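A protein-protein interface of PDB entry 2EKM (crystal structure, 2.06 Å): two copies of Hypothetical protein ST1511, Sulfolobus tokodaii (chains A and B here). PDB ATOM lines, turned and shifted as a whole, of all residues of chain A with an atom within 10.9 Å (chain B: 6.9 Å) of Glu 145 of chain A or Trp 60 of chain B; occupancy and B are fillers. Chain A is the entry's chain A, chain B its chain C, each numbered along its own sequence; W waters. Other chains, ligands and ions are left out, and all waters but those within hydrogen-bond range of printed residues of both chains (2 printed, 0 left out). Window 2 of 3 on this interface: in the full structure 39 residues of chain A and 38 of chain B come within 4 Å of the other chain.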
ATOM      1  N   PRO A 139      14.171   5.285 -17.779  1.00  0.00           N
ATOM      2  CA  PRO A 139      15.217   6.309 -17.893  1.00  0.00           C
ATOM      3  C   PRO A 139      16.030   6.536 -16.619  1.00  0.00           C
ATOM      4  O   PRO A 139      15.477   6.618 -15.526  1.00  0.00           O
ATOM      5  CB  PRO A 139      14.437   7.548 -18.324  1.00  0.00           C
ATOM      6  CG  PRO A 139      13.094   7.339 -17.684  1.00  0.00           C
ATOM      7  CD  PRO A 139      12.831   5.881 -17.942  1.00  0.00           C
ATOM      8  N   GLY A 141      18.313   9.179 -16.362  1.00  0.00           N
ATOM      9  CA  GLY A 141      18.774  10.554 -16.284  1.00  0.00           C
ATOM     10  C   GLY A 141      18.529  11.347 -17.554  1.00  0.00           C
ATOM     11  O   GLY A 141      17.847  10.879 -18.470  1.00  0.00           O
ATOM     12  N   ILE A 142      19.094  12.552 -17.604  1.00  0.00           N
ATOM     13  CA  ILE A 142      18.949  13.441 -18.753  1.00  0.00           C
ATOM     14  C   ILE A 142      20.311  13.645 -19.410  1.00  0.00           C
ATOM     15  O   ILE A 142      21.288  13.960 -18.732  1.00  0.00           O
ATOM     16  CB  ILE A 142      18.384  14.808 -18.315  1.00  0.00           C
ATOM     17  CG1 ILE A 142      17.034  14.607 -17.624  1.00  0.00           C
ATOM     18  CG2 ILE A 142      18.238  15.728 -19.522  1.00  0.00           C
ATOM     19  CD1 ILE A 142      16.416  15.881 -17.094  1.00  0.00           C
ATOM     20  N   GLU A 143      20.376  13.473 -20.729  1.00  0.00           N
ATOM     21  CA  GLU A 143      21.640  13.619 -21.442  1.00  0.00           C
ATOM     22  C   GLU A 143      22.169  15.048 -21.378  1.00  0.00           C
ATOM     23  O   GLU A 143      21.403  16.009 -21.328  1.00  0.00           O
ATOM     24  CB  GLU A 143      21.494  13.192 -22.909  1.00  0.00           C
ATOM     25  CG  GLU A 143      20.969  14.281 -23.837  1.00  0.00           C
ATOM     26  CD  GLU A 143      20.915  13.837 -25.288  1.00  0.00           C
ATOM     27  OE1 GLU A 143      21.886  13.205 -25.760  1.00  0.00           O
ATOM     28  OE2 GLU A 143      19.909  14.132 -25.962  1.00  0.00           O
ATOM     29  N   THR A 144      23.491  15.169 -21.386  1.00  0.00           N
ATOM     30  CA  THR A 144      24.162  16.463 -21.325  1.00  0.00           C
ATOM     31  C   THR A 144      24.591  16.901 -22.724  1.00  0.00           C
ATOM     32  O   THR A 144      24.418  16.164 -23.694  1.00  0.00           O
ATOM     33  CB  THR A 144      25.424  16.383 -20.455  1.00  0.00           C
ATOM     34  OG1 THR A 144      26.377  15.515 -21.089  1.00  0.00           O
ATOM     35  CG2 THR A 144      25.088  15.826 -19.072  1.00  0.00           C
ATOM     36  N   GLU A 145      25.158  18.100 -22.820  1.00  0.00           N
ATOM     37  CA  GLU A 145      25.630  18.614 -24.100  1.00  0.00           C
ATOM     38  C   GLU A 145      26.667  17.647 -24.651  1.00  0.00           C
ATOM     39  O   GLU A 145      26.707  17.377 -25.852  1.00  0.00           O
ATOM     40  CB  GLU A 145      26.253  20.001 -23.928  1.00  0.00           C
ATOM     41  CG  GLU A 145      25.251  21.127 -23.732  1.00  0.00           C
ATOM     42  CD  GLU A 145      24.287  21.266 -24.901  1.00  0.00           C
ATOM     43  OE1 GLU A 145      24.675  20.914 -26.038  1.00  0.00           O
ATOM     44  OE2 GLU A 145      23.149  21.739 -24.689  1.00  0.00           O
ATOM     45  N   ALA A 146      27.503  17.120 -23.761  1.00  0.00           N
ATOM     46  CA  ALA A 146      28.535  16.168 -24.154  1.00  0.00           C
ATOM     47  C   ALA A 146      27.878  14.939 -24.776  1.00  0.00           C
ATOM     48  O   ALA A 146      28.322  14.457 -25.817  1.00  0.00           O
ATOM     49  CB  ALA A 146      29.368  15.763 -22.941  1.00  0.00           C
ATOM     50  N   ASP A 147      26.824  14.436 -24.134  1.00  0.00           N
ATOM     51  CA  ASP A 147      26.099  13.270 -24.641  1.00  0.00           C
ATOM     52  C   ASP A 147      25.529  13.573 -26.025  1.00  0.00           C
ATOM     53  O   ASP A 147      25.614  12.756 -26.940  1.00  0.00           O
ATOM     54  CB  ASP A 147      24.943  12.892 -23.703  1.00  0.00           C
ATOM     55  CG  ASP A 147      25.418  12.370 -22.358  1.00  0.00           C
ATOM     56  OD1 ASP A 147      26.397  11.595 -22.335  1.00  0.00           O
ATOM     57  OD2 ASP A 147      24.798  12.719 -21.327  1.00  0.00           O
ATOM     58  N   ILE A 148      24.943  14.756 -26.162  1.00  0.00           N
ATOM     59  CA  ILE A 148      24.352  15.193 -27.419  1.00  0.00           C
ATOM     60  C   ILE A 148      25.372  15.151 -28.554  1.00  0.00           C
ATOM     61  O   ILE A 148      25.080  14.672 -29.650  1.00  0.00           O
ATOM     62  CB  ILE A 148      23.797  16.629 -27.284  1.00  0.00           C
ATOM     63  CG1 ILE A 148      22.624  16.630 -26.296  1.00  0.00           C
ATOM     64  CG2 ILE A 148      23.378  17.166 -28.649  1.00  0.00           C
ATOM     65  CD1 ILE A 148      22.026  18.003 -26.045  1.00  0.00           C
ATOM     66  N   LYS A 149      26.572  15.650 -28.282  1.00  0.00           N
ATOM     67  CA  LYS A 149      27.633  15.670 -29.279  1.00  0.00           C
ATOM     68  C   LYS A 149      27.978  14.253 -29.726  1.00  0.00           C
ATOM     69  O   LYS A 149      28.255  14.009 -30.902  1.00  0.00           O
ATOM     70  CB  LYS A 149      28.872  16.363 -28.701  1.00  0.00           C
ATOM     71  CG  LYS A 149      30.079  16.390 -29.619  1.00  0.00           C
ATOM     72  CD  LYS A 149      31.184  17.251 -29.020  1.00  0.00           C
ATOM     73  CE  LYS A 149      32.454  17.194 -29.857  1.00  0.00           C
ATOM     74  NZ  LYS A 149      33.028  15.822 -29.882  1.00  0.00           N
ATOM     75  N   GLU A 150      27.941  13.313 -28.789  1.00  0.00           N
ATOM     76  CA  GLU A 150      28.268  11.933 -29.107  1.00  0.00           C
ATOM     77  C   GLU A 150      27.199  11.209 -29.933  1.00  0.00           C
ATOM     78  O   GLU A 150      27.533  10.472 -30.858  1.00  0.00           O
ATOM     79  CB  GLU A 150      28.552  11.151 -27.826  1.00  0.00           C
ATOM     80  CG  GLU A 150      29.125   9.768 -28.081  1.00  0.00           C
ATOM     81  CD  GLU A 150      29.569   9.075 -26.810  1.00  0.00           C
ATOM     82  OE1 GLU A 150      30.316   9.699 -26.026  1.00  0.00           O
ATOM     83  OE2 GLU A 150      29.179   7.904 -26.601  1.00  0.00           O
ATOM     84  N   ARG A 151      25.922  11.408 -29.614  1.00  0.00           N
ATOM     85  CA  ARG A 151      24.881  10.734 -30.383  1.00  0.00           C
ATOM     86  C   ARG A 151      24.818  11.293 -31.804  1.00  0.00           C
ATOM     87  O   ARG A 151      24.440  10.587 -32.742  1.00  0.00           O
ATOM     88  CB  ARG A 151      23.514  10.842 -29.696  1.00  0.00           C
ATOM     89  CG  ARG A 151      22.910  12.232 -29.583  1.00  0.00           C
ATOM     90  CD  ARG A 151      21.486  12.103 -29.044  1.00  0.00           C
ATOM     91  NE  ARG A 151      20.873  13.372 -28.660  1.00  0.00           N
ATOM     92  CZ  ARG A 151      20.529  14.335 -29.507  1.00  0.00           C
ATOM     93  NH1 ARG A 151      20.732  14.187 -30.811  1.00  0.00           N
ATOM     94  NH2 ARG A 151      19.973  15.449 -29.045  1.00  0.00           N
ATOM     95  N   LYS A 152      25.195  12.559 -31.962  1.00  0.00           N
ATOM     96  CA  LYS A 152      25.213  13.171 -33.284  1.00  0.00           C
ATOM     97  C   LYS A 152      26.312  12.491 -34.100  1.00  0.00           C
ATOM     98  O   LYS A 152      26.092  12.090 -35.244  1.00  0.00           O
ATOM     99  CB  LYS A 152      25.485  14.674 -33.182  1.00  0.00           C
ATOM    100  CG  LYS A 152      24.299  15.478 -32.666  1.00  0.00           C
ATOM    101  CD  LYS A 152      24.602  16.968 -32.611  1.00  0.00           C
ATOM    102  CE  LYS A 152      23.404  17.746 -32.090  1.00  0.00           C
ATOM    103  NZ  LYS A 152      23.723  19.179 -31.842  1.00  0.00           N
ATOM    104  N   GLU A 153      27.490  12.347 -33.499  1.00  0.00           N
ATOM    105  CA  GLU A 153      28.609  11.697 -34.179  1.00  0.00           C
ATOM    106  C   GLU A 153      28.244  10.257 -34.520  1.00  0.00           C
ATOM    107  O   GLU A 153      28.622   9.733 -35.568  1.00  0.00           O
ATOM    108  CB  GLU A 153      29.855  11.712 -33.289  1.00  0.00           C
ATOM    109  CG  GLU A 153      30.280  13.105 -32.859  1.00  0.00           C
ATOM    110  CD  GLU A 153      31.604  13.113 -32.119  1.00  0.00           C
ATOM    111  OE1 GLU A 153      31.765  12.313 -31.171  1.00  0.00           O
ATOM    112  OE2 GLU A 153      32.480  13.927 -32.483  1.00  0.00           O
ATOM    113  N   LEU A 155      25.274   8.874 -35.332  1.00  0.00           N
ATOM    114  CA  LEU A 155      24.456   8.761 -36.537  1.00  0.00           C
ATOM    115  C   LEU A 155      25.255   9.057 -37.803  1.00  0.00           C
ATOM    116  O   LEU A 155      25.017   8.459 -38.851  1.00  0.00           O
ATOM    117  CB  LEU A 155      23.251   9.700 -36.456  1.00  0.00           C
ATOM    118  CG  LEU A 155      22.248   9.402 -35.338  1.00  0.00           C
ATOM    119  CD1 LEU A 155      21.040  10.300 -35.496  1.00  0.00           C
ATOM    120  CD2 LEU A 155      21.832   7.939 -35.386  1.00  0.00           C
ATOM    121  N   VAL B  29      15.107  11.525 -31.946  1.00  0.00           N
ATOM    122  CA  VAL B  29      15.288  12.929 -31.588  1.00  0.00           C
ATOM    123  C   VAL B  29      15.579  13.877 -32.749  1.00  0.00           C
ATOM    124  O   VAL B  29      14.851  14.845 -32.941  1.00  0.00           O
ATOM    125  CB  VAL B  29      16.396  13.090 -30.526  1.00  0.00           C
ATOM    126  CG1 VAL B  29      16.515  14.555 -30.113  1.00  0.00           C
ATOM    127  CG2 VAL B  29      16.073  12.231 -29.318  1.00  0.00           C
ATOM    128  N   GLY B  46       9.643  21.488 -27.833  1.00  0.00           N
ATOM    129  CA  GLY B  46      10.605  20.813 -26.980  1.00  0.00           C
ATOM    130  C   GLY B  46      10.369  19.325 -27.166  1.00  0.00           C
ATOM    131  O   GLY B  46       9.218  18.887 -27.219  1.00  0.00           O
ATOM    132  N   ILE B  47      11.448  18.553 -27.256  1.00  0.00           N
ATOM    133  CA  ILE B  47      11.361  17.112 -27.482  1.00  0.00           C
ATOM    134  C   ILE B  47      12.189  16.289 -26.498  1.00  0.00           C
ATOM    135  O   ILE B  47      13.335  16.632 -26.211  1.00  0.00           O
ATOM    136  CB  ILE B  47      11.875  16.757 -28.898  1.00  0.00           C
ATOM    137  CG1 ILE B  47      11.143  17.597 -29.943  1.00  0.00           C
ATOM    138  CG2 ILE B  47      11.698  15.260 -29.162  1.00  0.00           C
ATOM    139  CD1 ILE B  47      11.820  17.590 -31.290  1.00  0.00           C
ATOM    140  N   ALA B  48      11.602  15.197 -26.006  1.00  0.00           N
ATOM    141  CA  ALA B  48      12.278  14.282 -25.087  1.00  0.00           C
ATOM    142  C   ALA B  48      11.986  12.843 -25.522  1.00  0.00           C
ATOM    143  O   ALA B  48      10.848  12.508 -25.856  1.00  0.00           O
ATOM    144  CB  ALA B  48      11.795  14.503 -23.652  1.00  0.00           C
ATOM    145  N   PHE B  49      13.014  11.999 -25.515  1.00  0.00           N
ATOM    146  CA  PHE B  49      12.878  10.598 -25.909  1.00  0.00           C
ATOM    147  C   PHE B  49      13.590   9.704 -24.900  1.00  0.00           C
ATOM    148  O   PHE B  49      14.746   9.952 -24.551  1.00  0.00           O
ATOM    149  CB  PHE B  49      13.481  10.387 -27.301  1.00  0.00           C
ATOM    150  CG  PHE B  49      13.551   8.946 -27.726  1.00  0.00           C
ATOM    151  CD1 PHE B  49      12.390   8.216 -27.970  1.00  0.00           C
ATOM    152  CD2 PHE B  49      14.782   8.318 -27.895  1.00  0.00           C
ATOM    153  CE1 PHE B  49      12.459   6.876 -28.380  1.00  0.00           C
ATOM    154  CE2 PHE B  49      14.862   6.979 -28.304  1.00  0.00           C
ATOM    155  CZ  PHE B  49      13.697   6.261 -28.545  1.00  0.00           C
ATOM    156  N   LEU B  57      19.339   7.190 -21.229  1.00  0.00           N
ATOM    157  CA  LEU B  57      19.195   8.626 -20.985  1.00  0.00           C
ATOM    158  C   LEU B  57      18.034   9.300 -21.705  1.00  0.00           C
ATOM    159  O   LEU B  57      17.662   8.918 -22.818  1.00  0.00           O
ATOM    160  CB  LEU B  57      20.487   9.349 -21.381  1.00  0.00           C
ATOM    161  CG  LEU B  57      21.755   8.955 -20.624  1.00  0.00           C
ATOM    162  CD1 LEU B  57      22.971   9.598 -21.281  1.00  0.00           C
ATOM    163  CD2 LEU B  57      21.633   9.379 -19.175  1.00  0.00           C
ATOM    164  N   ILE B  58      17.455  10.307 -21.056  1.00  0.00           N
ATOM    165  CA  ILE B  58      16.381  11.073 -21.669  1.00  0.00           C
ATOM    166  C   ILE B  58      17.097  11.911 -22.732  1.00  0.00           C
ATOM    167  O   ILE B  58      17.887  12.797 -22.397  1.00  0.00           O
ATOM    168  CB  ILE B  58      15.700  12.045 -20.667  1.00  0.00           C
ATOM    169  CG1 ILE B  58      14.989  11.271 -19.557  1.00  0.00           C
ATOM    170  CG2 ILE B  58      14.705  12.938 -21.405  1.00  0.00           C
ATOM    171  CD1 ILE B  58      13.812  10.450 -20.020  1.00  0.00           C
ATOM    172  N   ARG B  59      16.839  11.614 -24.002  1.00  0.00           N
ATOM    173  CA  ARG B  59      17.455  12.340 -25.111  1.00  0.00           C
ATOM    174  C   ARG B  59      16.524  13.484 -25.513  1.00  0.00           C
ATOM    175  O   ARG B  59      15.309  13.296 -25.629  1.00  0.00           O
ATOM    176  CB  ARG B  59      17.685  11.392 -26.288  1.00  0.00           C
ATOM    177  CG  ARG B  59      18.463  10.123 -25.915  1.00  0.00           C
ATOM    178  CD  ARG B  59      19.861  10.452 -25.404  1.00  0.00           C
ATOM    179  NE  ARG B  59      20.679   9.254 -25.215  1.00  0.00           N
ATOM    180  CZ  ARG B  59      22.000   9.226 -25.359  1.00  0.00           C
ATOM    181  NH1 ARG B  59      22.653  10.333 -25.690  1.00  0.00           N
ATOM    182  NH2 ARG B  59      22.670   8.093 -25.191  1.00  0.00           N
ATOM    183  N   TRP B  60      17.090  14.667 -25.740  1.00  0.00           N
ATOM    184  CA  TRP B  60      16.268  15.828 -26.066  1.00  0.00           C
ATOM    185  C   TRP B  60      16.850  16.804 -27.077  1.00  0.00           C
ATOM    186  O   TRP B  60      18.029  16.752 -27.414  1.00  0.00           O
ATOM    187  CB  TRP B  60      15.971  16.612 -24.784  1.00  0.00           C
ATOM    188  CG  TRP B  60      17.228  16.976 -24.049  1.00  0.00           C
ATOM    189  CD1 TRP B  60      17.925  16.188 -23.180  1.00  0.00           C
ATOM    190  CD2 TRP B  60      17.993  18.181 -24.197  1.00  0.00           C
ATOM    191  NE1 TRP B  60      19.076  16.822 -22.779  1.00  0.00           N
ATOM    192  CE2 TRP B  60      19.143  18.048 -23.388  1.00  0.00           C
ATOM    193  CE3 TRP B  60      17.818  19.360 -24.937  1.00  0.00           C
ATOM    194  CZ2 TRP B  60      20.119  19.051 -23.297  1.00  0.00           C
ATOM    195  CZ3 TRP B  60      18.791  20.359 -24.847  1.00  0.00           C
ATOM    196  CH2 TRP B  60      19.926  20.194 -24.031  1.00  0.00           C
ATOM    197  N   ASP B  61      15.984  17.705 -27.533  1.00  0.00           N
ATOM    198  CA  ASP B  61      16.338  18.761 -28.469  1.00  0.00           C
ATOM    199  C   ASP B  61      15.099  19.639 -28.639  1.00  0.00           C
ATOM    200  O   ASP B  61      14.043  19.355 -28.061  1.00  0.00           O
ATOM    201  CB  ASP B  61      16.763  18.189 -29.821  1.00  0.00           C
ATOM    202  CG  ASP B  61      17.702  19.120 -30.575  1.00  0.00           C
ATOM    203  OD1 ASP B  61      17.682  20.339 -30.308  1.00  0.00           O
ATOM    204  OD2 ASP B  61      18.458  18.633 -31.438  1.00  0.00           O
ATOM    205  N   GLY B  62      15.227  20.698 -29.430  1.00  0.00           N
ATOM    206  CA  GLY B  62      14.114  21.601 -29.653  1.00  0.00           C
ATOM    207  C   GLY B  62      14.632  23.015 -29.830  1.00  0.00           C
ATOM    208  O   GLY B  62      15.843  23.227 -29.879  1.00  0.00           O
ATOM    209  N   GLU B  65      13.828  26.133 -24.724  1.00  0.00           N
ATOM    210  CA  GLU B  65      14.263  25.483 -23.490  1.00  0.00           C
ATOM    211  C   GLU B  65      13.141  25.204 -22.486  1.00  0.00           C
ATOM    212  O   GLU B  65      13.129  24.156 -21.847  1.00  0.00           O
ATOM    213  CB  GLU B  65      15.358  26.321 -22.824  1.00  0.00           C
ATOM    214  CG  GLU B  65      16.066  25.630 -21.666  1.00  0.00           C
ATOM    215  CD  GLU B  65      16.601  24.255 -22.037  1.00  0.00           C
ATOM    216  OE1 GLU B  65      17.070  24.088 -23.185  1.00  0.00           O
ATOM    217  OE2 GLU B  65      16.565  23.347 -21.175  1.00  0.00           O
ATOM    218  N   ILE B  68      11.417  22.267 -23.683  1.00  0.00           N
ATOM    219  CA  ILE B  68      12.322  21.128 -23.584  1.00  0.00           C
ATOM    220  C   ILE B  68      12.324  20.571 -22.164  1.00  0.00           C
ATOM    221  O   ILE B  68      12.276  19.355 -21.965  1.00  0.00           O
ATOM    222  CB  ILE B  68      13.768  21.531 -23.959  1.00  0.00           C
ATOM    223  CG1 ILE B  68      13.893  21.673 -25.477  1.00  0.00           C
ATOM    224  CG2 ILE B  68      14.763  20.493 -23.439  1.00  0.00           C
ATOM    225  CD1 ILE B  68      15.265  22.174 -25.929  1.00  0.00           C
ATOM    226  N   ALA B  71       9.240  18.736 -21.430  1.00  0.00           N
ATOM    227  CA  ALA B  71       9.253  17.441 -22.104  1.00  0.00           C
ATOM    228  C   ALA B  71      10.070  16.436 -21.302  1.00  0.00           C
ATOM    229  O   ALA B  71       9.669  15.283 -21.144  1.00  0.00           O
ATOM    230  CB  ALA B  71       9.830  17.587 -23.515  1.00  0.00           C
ATOM    231  N   GLN B  72      11.215  16.886 -20.795  1.00  0.00           N
ATOM    232  CA  GLN B  72      12.095  16.034 -20.005  1.00  0.00           C
ATOM    233  C   GLN B  72      11.391  15.589 -18.723  1.00  0.00           C
ATOM    234  O   GLN B  72      11.477  14.428 -18.330  1.00  0.00           O
ATOM    235  CB  GLN B  72      13.387  16.781 -19.636  1.00  0.00           C
ATOM    236  CG  GLN B  72      14.222  17.273 -20.815  1.00  0.00           C
ATOM    237  CD  GLN B  72      15.405  18.120 -20.361  1.00  0.00           C
ATOM    238  OE1 GLN B  72      15.297  18.877 -19.398  1.00  0.00           O
ATOM    239  NE2 GLN B  72      16.527  18.006 -21.057  1.00  0.00           N
HETATM  240  O   HOH W   1      25.451  10.007 -26.428  1.00  0.00           O
HETATM  241  O   HOH W   2      21.305  19.909 -30.566  1.00  0.00           O
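NH2 of Arg 151 of chain A sits at hydrogen-bond distance from O of Trp 60 of chain B, at 2.9 Å.
O of Ile 58 of chain B lies within hydrogen-bond range of N of Glu 143 of chain A (3.1 Å).
The backbone NH of Ile 58 of chain B lies within hydrogen-bond range of the backbone carbonyl oxygen of Gly 141 of chain A (2.7 Å).
The indole nitrogen (NE1) of Trp 60 of chain B lies within hydrogen-bond range of the backbone carbonyl oxygen (O) of Glu 143 of chain A.
The side-chain carboxylate (OE1) of Glu 143 of chain A is in salt-bridge range of the guanidinium group (NH1) of Arg 59 of chain B, at 3.0 Å.
The side-chain carboxylate (OE2) of Glu 143 of chain A lies within salt-bridge range of the guanidinium group (NE) of Arg 151 of chain A (3.0 Å).
O of Arg 59 of chain B lies within hydrogen-bond range of N of Phe 49 of chain B (2.6 Å).
The indole nitrogen of Trp 60 of chain B lies close to the side-chain amide nitrogen of Gln 72 of chain B (3.3 Å).
The side-chain carboxylate (OE1) of Glu 143 of chain A is in hydrogen-bond range of the backbone NH (N) of Ile 148 of chain A (3.5 Å).
The backbone NH (N) of Thr 144 of chain A sits at hydrogen-bond distance from the side-chain carboxylate (OD2) of Asp 147 of chain A (2.8 Å).
Among the printed residues, pairs that only touch across the chains: Pro 139 of chain A with Ile 58 of chain B, Gly 141 of chain A with Leu 57 of chain B, Ile 142 of chain A with Ile 58 of chain B, Ile 142 of chain A with Trp 60 of chain B, Ile 142 of chain A with Gln 72 of chain B, Glu 145 of chain A with Trp 60 of chain B, Asp 147 of chain A with Leu 57 of chain B, Asp 147 of chain A with Arg 59 of chain B, Ile 148 of chain A with Trp 60 of chain B, Arg 151 of chain A with Val 29 of chain B and Arg 151 of chain A with Arg 59 of chain B.
Of chain B, only Trp 60 (3.6 Å) comes within 4 Å of Glu 145 of chain A.
Trp 60 of chain B touches just these residues of chain A: Ile 142 (3.5 Å), Glu 143 (2.9 Å), Glu 145 (3.6 Å), Ile 148 (3.5 Å) and Arg 151 (2.9 Å).
No residue of chain A comes within 4 Å of Ile 47 of chain B.
Asp 61 of chain B touches none of the printed residues of chain A.
Of the printed residues of chain B, Ile 142 of chain A touches Ile 58, Trp 60 and Gln 72.
Printed residues of chain A within 4 Å of Arg 59 of chain B: Glu 143 (3.0 Å), Asp 147 (3.97 Å) and Arg 151 (3.97 Å).
Printed residues of chain B within 4 Å of Pro 139 of chain A: Ile 58 (3.4 Å).
Of the printed residues of chain A, Leu 57 of chain B touches Gly 141 and Asp 147.
The nearest residue of chain B that does not touch Glu 145 of chain A is Glu 65 of chain B (6.7 Å).
The nearest residue of chain A that does not touch Trp 60 of chain B is Thr 144 of chain A (4.9 Å).
The nearest printed residue of chain B that does not touch Asp 147 of chain A is Ile 58 of chain B (7.0 Å).
Along chain A the printed residues that touch a printed residue of chain B span positions 139 to 151.
Of the 15 printed residues of chain B, 6 touch a printed residue of chain A.
Among the printed residues, Asp or Glu carboxylates within 4 Å of a Lys or Arg side-chain nitrogen of the other chain: Glu 143 of chain A with Arg 59 of chain B (3.0 Å).
No position is printed for both chains.
Water W1 lies within hydrogen-bond range of the backbone carbonyl oxygen (O) of Asp 147 of chain A (2.8 Å) and the guanidinium group (NH1) of Arg 59 of chain B (2.9 Å).
Water W2 bridges the side-chain amino group (NZ) of Lys 152 of chain A and the side-chain carboxylate (OD2) of Asp 61 of chain B.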
